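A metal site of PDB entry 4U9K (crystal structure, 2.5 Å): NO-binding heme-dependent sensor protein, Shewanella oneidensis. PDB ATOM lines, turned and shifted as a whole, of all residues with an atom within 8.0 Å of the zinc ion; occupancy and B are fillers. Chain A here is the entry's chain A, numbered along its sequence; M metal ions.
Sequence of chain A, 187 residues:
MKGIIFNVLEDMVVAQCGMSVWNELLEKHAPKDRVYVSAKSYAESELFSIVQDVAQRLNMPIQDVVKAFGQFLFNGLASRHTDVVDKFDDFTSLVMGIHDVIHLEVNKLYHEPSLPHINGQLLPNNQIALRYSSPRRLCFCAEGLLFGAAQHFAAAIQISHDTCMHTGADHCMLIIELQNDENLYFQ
The zinc ion is bound by NE2 of His 161 (2.0 Å), SG of Cys 172 (2.3 Å), SG of Cys 139 (2.3 Å) and SG of Cys 164 (2.3 Å).
Merely in contact with the zinc ion: Met 165.
The nearest printed residue that does not touch the zinc ion is Thr 163 (4.5 Å).
A ring nitrogen (ND1) of His 161 lies within hydrogen-bond range of the side-chain carboxylate of Glu 143, at 2.8 Å.
The side-chain sulfur of Cys 172 sits close to the backbone NH of Met 165, at 3.3 Å.
N of Cys 172 sits at hydrogen-bond distance from O of Tyr 132, 2.8 Å away.
The backbone NH (N) of His 166 sits close to the side-chain sulfur (SG) of Cys 164 (3.3 Å).
O of Cys 164 lies within hydrogen-bond range of OG1 of Thr 167 (3.2 Å).
The backbone carbonyl oxygen (O) of Cys 164 lies within hydrogen-bond range of the backbone NH (N) of Ala 169 (3.1 Å).
The guanidinium group of Arg 137 lies within hydrogen-bond range of the backbone carbonyl oxygen of Met 165.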
ATOM      1  N   TYR A 132      -8.307  -8.322  28.294  1.00  0.00           N
ATOM      2  CA  TYR A 132      -9.646  -8.703  27.855  1.00  0.00           C
ATOM      3  C   TYR A 132      -9.579  -9.318  26.495  1.00  0.00           C
ATOM      4  O   TYR A 132      -8.748  -8.984  25.686  1.00  0.00           O
ATOM      5  CB  TYR A 132     -10.573  -7.496  27.845  1.00  0.00           C
ATOM      6  CG  TYR A 132     -11.851  -7.615  27.097  1.00  0.00           C
ATOM      7  CD1 TYR A 132     -11.910  -7.426  25.748  1.00  0.00           C
ATOM      8  CD2 TYR A 132     -13.017  -7.834  27.743  1.00  0.00           C
ATOM      9  CE1 TYR A 132     -13.125  -7.518  25.055  1.00  0.00           C
ATOM     10  CE2 TYR A 132     -14.237  -7.909  27.063  1.00  0.00           C
ATOM     11  CZ  TYR A 132     -14.270  -7.757  25.712  1.00  0.00           C
ATOM     12  OH  TYR A 132     -15.461  -7.823  25.029  1.00  0.00           O
ATOM     13  N   ARG A 137     -15.857  -8.146  21.121  1.00  0.00           N
ATOM     14  CA  ARG A 137     -15.071  -6.942  21.091  1.00  0.00           C
ATOM     15  C   ARG A 137     -15.718  -5.801  21.823  1.00  0.00           C
ATOM     16  O   ARG A 137     -15.813  -4.688  21.299  1.00  0.00           O
ATOM     17  CB  ARG A 137     -14.802  -6.552  19.636  1.00  0.00           C
ATOM     18  CG  ARG A 137     -13.983  -7.623  18.920  1.00  0.00           C
ATOM     19  CD  ARG A 137     -13.013  -7.038  17.858  1.00  0.00           C
ATOM     20  NE  ARG A 137     -13.777  -6.559  16.725  1.00  0.00           N
ATOM     21  CZ  ARG A 137     -13.228  -6.045  15.634  1.00  0.00           C
ATOM     22  NH1 ARG A 137     -11.919  -5.906  15.542  1.00  0.00           N
ATOM     23  NH2 ARG A 137     -14.021  -5.639  14.660  1.00  0.00           N
ATOM     24  N   LEU A 138     -16.128  -6.050  23.056  1.00  0.00           N
ATOM     25  CA  LEU A 138     -16.812  -5.041  23.865  1.00  0.00           C
ATOM     26  C   LEU A 138     -15.924  -4.495  24.948  1.00  0.00           C
ATOM     27  O   LEU A 138     -16.376  -4.273  26.072  1.00  0.00           O
ATOM     28  CB  LEU A 138     -18.086  -5.625  24.481  1.00  0.00           C
ATOM     29  CG  LEU A 138     -19.170  -5.907  23.419  1.00  0.00           C
ATOM     30  CD1 LEU A 138     -20.270  -6.833  24.031  1.00  0.00           C
ATOM     31  CD2 LEU A 138     -19.773  -4.571  23.021  1.00  0.00           C
ATOM     32  N   CYS A 139     -14.680  -4.216  24.588  1.00  0.00           N
ATOM     33  CA  CYS A 139     -13.711  -3.689  25.533  1.00  0.00           C
ATOM     34  C   CYS A 139     -14.153  -2.312  26.045  1.00  0.00           C
ATOM     35  O   CYS A 139     -13.811  -1.928  27.155  1.00  0.00           O
ATOM     36  CB  CYS A 139     -12.339  -3.553  24.899  1.00  0.00           C
ATOM     37  SG  CYS A 139     -12.362  -2.586  23.316  1.00  0.00           S
ATOM     38  N   PHE A 140     -14.925  -1.563  25.272  1.00  0.00           N
ATOM     39  CA  PHE A 140     -15.342  -0.263  25.801  1.00  0.00           C
ATOM     40  C   PHE A 140     -16.462  -0.397  26.787  1.00  0.00           C
ATOM     41  O   PHE A 140     -16.617   0.429  27.683  1.00  0.00           O
ATOM     42  CB  PHE A 140     -15.716   0.701  24.683  1.00  0.00           C
ATOM     43  CG  PHE A 140     -14.526   1.208  23.980  1.00  0.00           C
ATOM     44  CD1 PHE A 140     -13.863   2.329  24.445  1.00  0.00           C
ATOM     45  CD2 PHE A 140     -14.025   0.544  22.886  1.00  0.00           C
ATOM     46  CE1 PHE A 140     -12.705   2.809  23.786  1.00  0.00           C
ATOM     47  CE2 PHE A 140     -12.900   0.991  22.250  1.00  0.00           C
ATOM     48  CZ  PHE A 140     -12.228   2.125  22.702  1.00  0.00           C
ATOM     49  N   ALA A 142     -16.422  -2.868  28.745  1.00  0.00           N
ATOM     50  CA  ALA A 142     -15.651  -3.252  29.931  1.00  0.00           C
ATOM     51  C   ALA A 142     -15.049  -2.055  30.666  1.00  0.00           C
ATOM     52  O   ALA A 142     -14.985  -2.076  31.903  1.00  0.00           O
ATOM     53  CB  ALA A 142     -14.572  -4.196  29.569  1.00  0.00           C
ATOM     54  N   GLU A 143     -14.606  -1.027  29.924  1.00  0.00           N
ATOM     55  CA  GLU A 143     -14.138   0.232  30.565  1.00  0.00           C
ATOM     56  C   GLU A 143     -15.246   0.891  31.377  1.00  0.00           C
ATOM     57  O   GLU A 143     -15.055   1.260  32.526  1.00  0.00           O
ATOM     58  CB  GLU A 143     -13.643   1.253  29.551  1.00  0.00           C
ATOM     59  CG  GLU A 143     -12.201   1.127  29.190  1.00  0.00           C
ATOM     60  CD  GLU A 143     -11.642   2.411  28.564  1.00  0.00           C
ATOM     61  OE1 GLU A 143     -10.994   2.228  27.488  1.00  0.00           O
ATOM     62  OE2 GLU A 143     -11.807   3.559  29.083  1.00  0.00           O
ATOM     63  N   HIS A 161      -5.714   2.169  27.459  1.00  0.00           N
ATOM     64  CA  HIS A 161      -6.258   1.153  26.600  1.00  0.00           C
ATOM     65  C   HIS A 161      -5.509   1.233  25.258  1.00  0.00           C
ATOM     66  O   HIS A 161      -6.070   1.653  24.237  1.00  0.00           O
ATOM     67  CB  HIS A 161      -7.766   1.387  26.457  1.00  0.00           C
ATOM     68  CG  HIS A 161      -8.534   0.319  25.753  1.00  0.00           C
ATOM     69  ND1 HIS A 161      -9.907   0.230  25.836  1.00  0.00           N
ATOM     70  CD2 HIS A 161      -8.142  -0.672  24.901  1.00  0.00           C
ATOM     71  CE1 HIS A 161     -10.328  -0.779  25.083  1.00  0.00           C
ATOM     72  NE2 HIS A 161      -9.278  -1.345  24.514  1.00  0.00           N
ATOM     73  N   ASP A 162      -4.241   0.825  25.265  1.00  0.00           N
ATOM     74  CA  ASP A 162      -3.377   1.003  24.101  1.00  0.00           C
ATOM     75  C   ASP A 162      -3.031  -0.274  23.309  1.00  0.00           C
ATOM     76  O   ASP A 162      -2.334  -0.204  22.331  1.00  0.00           O
ATOM     77  CB  ASP A 162      -2.065   1.671  24.511  1.00  0.00           C
ATOM     78  CG  ASP A 162      -2.257   3.096  25.115  1.00  0.00           C
ATOM     79  OD1 ASP A 162      -2.935   3.952  24.468  1.00  0.00           O
ATOM     80  OD2 ASP A 162      -1.687   3.388  26.212  1.00  0.00           O
ATOM     81  N   THR A 163      -3.458  -1.407  23.752  1.00  0.00           N
ATOM     82  CA  THR A 163      -3.525  -2.589  22.928  1.00  0.00           C
ATOM     83  C   THR A 163      -4.992  -2.862  22.856  1.00  0.00           C
ATOM     84  O   THR A 163      -5.672  -2.900  23.910  1.00  0.00           O
ATOM     85  CB  THR A 163      -2.781  -3.751  23.582  1.00  0.00           C
ATOM     86  OG1 THR A 163      -1.444  -3.320  23.850  1.00  0.00           O
ATOM     87  CG2 THR A 163      -2.742  -4.960  22.725  1.00  0.00           C
ATOM     88  N   CYS A 164      -5.510  -3.050  21.633  1.00  0.00           N
ATOM     89  CA  CYS A 164      -6.958  -3.146  21.452  1.00  0.00           C
ATOM     90  C   CYS A 164      -7.292  -4.036  20.264  1.00  0.00           C
ATOM     91  O   CYS A 164      -6.555  -4.049  19.262  1.00  0.00           O
ATOM     92  CB  CYS A 164      -7.604  -1.750  21.305  1.00  0.00           C
ATOM     93  SG  CYS A 164      -9.372  -1.791  21.164  1.00  0.00           S
ATOM     94  N   MET A 165      -8.402  -4.789  20.382  1.00  0.00           N
ATOM     95  CA  MET A 165      -8.840  -5.669  19.306  1.00  0.00           C
ATOM     96  C   MET A 165      -9.261  -4.770  18.122  1.00  0.00           C
ATOM     97  O   MET A 165      -9.107  -5.145  16.937  1.00  0.00           O
ATOM     98  CB  MET A 165      -9.944  -6.627  19.773  1.00  0.00           C
ATOM     99  CG  MET A 165      -9.556  -7.571  20.937  1.00  0.00           C
ATOM    100  SD  MET A 165     -10.867  -8.744  21.424  1.00  0.00           S
ATOM    101  CE  MET A 165     -10.738  -9.788  19.975  1.00  0.00           C
ATOM    102  N   HIS A 166      -9.720  -3.560  18.405  1.00  0.00           N
ATOM    103  CA  HIS A 166     -10.134  -2.654  17.344  1.00  0.00           C
ATOM    104  C   HIS A 166      -8.970  -2.063  16.581  1.00  0.00           C
ATOM    105  O   HIS A 166      -9.186  -1.467  15.549  1.00  0.00           O
ATOM    106  CB  HIS A 166     -11.032  -1.543  17.904  1.00  0.00           C
ATOM    107  CG  HIS A 166     -12.338  -2.050  18.401  1.00  0.00           C
ATOM    108  ND1 HIS A 166     -13.335  -2.475  17.538  1.00  0.00           N
ATOM    109  CD2 HIS A 166     -12.807  -2.278  19.645  1.00  0.00           C
ATOM    110  CE1 HIS A 166     -14.356  -2.918  18.249  1.00  0.00           C
ATOM    111  NE2 HIS A 166     -14.061  -2.814  19.520  1.00  0.00           N
ATOM    112  N   THR A 167      -7.730  -2.249  17.060  1.00  0.00           N
ATOM    113  CA  THR A 167      -6.526  -1.746  16.331  1.00  0.00           C
ATOM    114  C   THR A 167      -5.638  -2.910  15.948  1.00  0.00           C
ATOM    115  O   THR A 167      -4.442  -2.753  15.700  1.00  0.00           O
ATOM    116  CB  THR A 167      -5.676  -0.707  17.141  1.00  0.00           C
ATOM    117  OG1 THR A 167      -5.190  -1.269  18.377  1.00  0.00           O
ATOM    118  CG2 THR A 167      -6.505   0.522  17.442  1.00  0.00           C
ATOM    119  N   ALA A 169      -5.135  -6.172  17.478  1.00  0.00           N
ATOM    120  CA  ALA A 169      -4.598  -7.173  18.387  1.00  0.00           C
ATOM    121  C   ALA A 169      -5.661  -8.239  18.601  1.00  0.00           C
ATOM    122  O   ALA A 169      -6.831  -8.030  18.256  1.00  0.00           O
ATOM    123  CB  ALA A 169      -4.197  -6.541  19.661  1.00  0.00           C
ATOM    124  N   HIS A 171      -6.345  -9.272  21.663  1.00  0.00           N
ATOM    125  CA  HIS A 171      -6.876  -8.954  23.019  1.00  0.00           C
ATOM    126  C   HIS A 171      -6.774  -7.458  23.237  1.00  0.00           C
ATOM    127  O   HIS A 171      -6.178  -6.754  22.400  1.00  0.00           O
ATOM    128  CB  HIS A 171      -6.055  -9.683  24.051  1.00  0.00           C
ATOM    129  CG  HIS A 171      -4.636  -9.224  24.103  1.00  0.00           C
ATOM    130  ND1 HIS A 171      -3.710  -9.601  23.150  1.00  0.00           N
ATOM    131  CD2 HIS A 171      -3.990  -8.387  24.948  1.00  0.00           C
ATOM    132  CE1 HIS A 171      -2.539  -9.046  23.427  1.00  0.00           C
ATOM    133  NE2 HIS A 171      -2.684  -8.299  24.503  1.00  0.00           N
ATOM    134  N   CYS A 172      -7.304  -6.973  24.352  1.00  0.00           N
ATOM    135  CA  CYS A 172      -7.016  -5.612  24.814  1.00  0.00           C
ATOM    136  C   CYS A 172      -6.293  -5.622  26.169  1.00  0.00           C
ATOM    137  O   CYS A 172      -6.485  -6.527  26.956  1.00  0.00           O
ATOM    138  CB  CYS A 172      -8.332  -4.789  24.969  1.00  0.00           C
ATOM    139  SG  CYS A 172      -9.488  -4.787  23.512  1.00  0.00           S
ATOM    140  N   MET A 173      -5.449  -4.629  26.440  1.00  0.00           N
ATOM    141  CA  MET A 173      -4.874  -4.433  27.759  1.00  0.00           C
ATOM    142  C   MET A 173      -5.462  -3.180  28.345  1.00  0.00           C
ATOM    143  O   MET A 173      -5.319  -2.098  27.796  1.00  0.00           O
ATOM    144  CB  MET A 173      -3.360  -4.347  27.707  1.00  0.00           C
ATOM    145  CG  MET A 173      -2.669  -5.648  27.318  1.00  0.00           C
ATOM    146  SD  MET A 173      -3.154  -7.117  28.298  1.00  0.00           S
ATOM    147  CE  MET A 173      -2.478  -6.648  29.882  1.00  0.00           C
ATOM    148  N   LEU A 174      -6.201  -3.335  29.444  1.00  0.00           N
ATOM    149  CA  LEU A 174      -6.724  -2.177  30.168  1.00  0.00           C
ATOM    150  C   LEU A 174      -5.803  -1.986  31.373  1.00  0.00           C
ATOM    151  O   LEU A 174      -5.777  -2.791  32.270  1.00  0.00           O
ATOM    152  CB  LEU A 174      -8.182  -2.415  30.579  1.00  0.00           C
ATOM    153  CG  LEU A 174      -9.218  -2.107  29.512  1.00  0.00           C
ATOM    154  CD1 LEU A 174      -8.807  -2.767  28.281  1.00  0.00           C
ATOM    155  CD2 LEU A 174     -10.503  -2.730  29.860  1.00  0.00           C
HETATM  156 ZN    ZN M   1     -10.075  -2.615  23.193  1.00  0.00          ZN
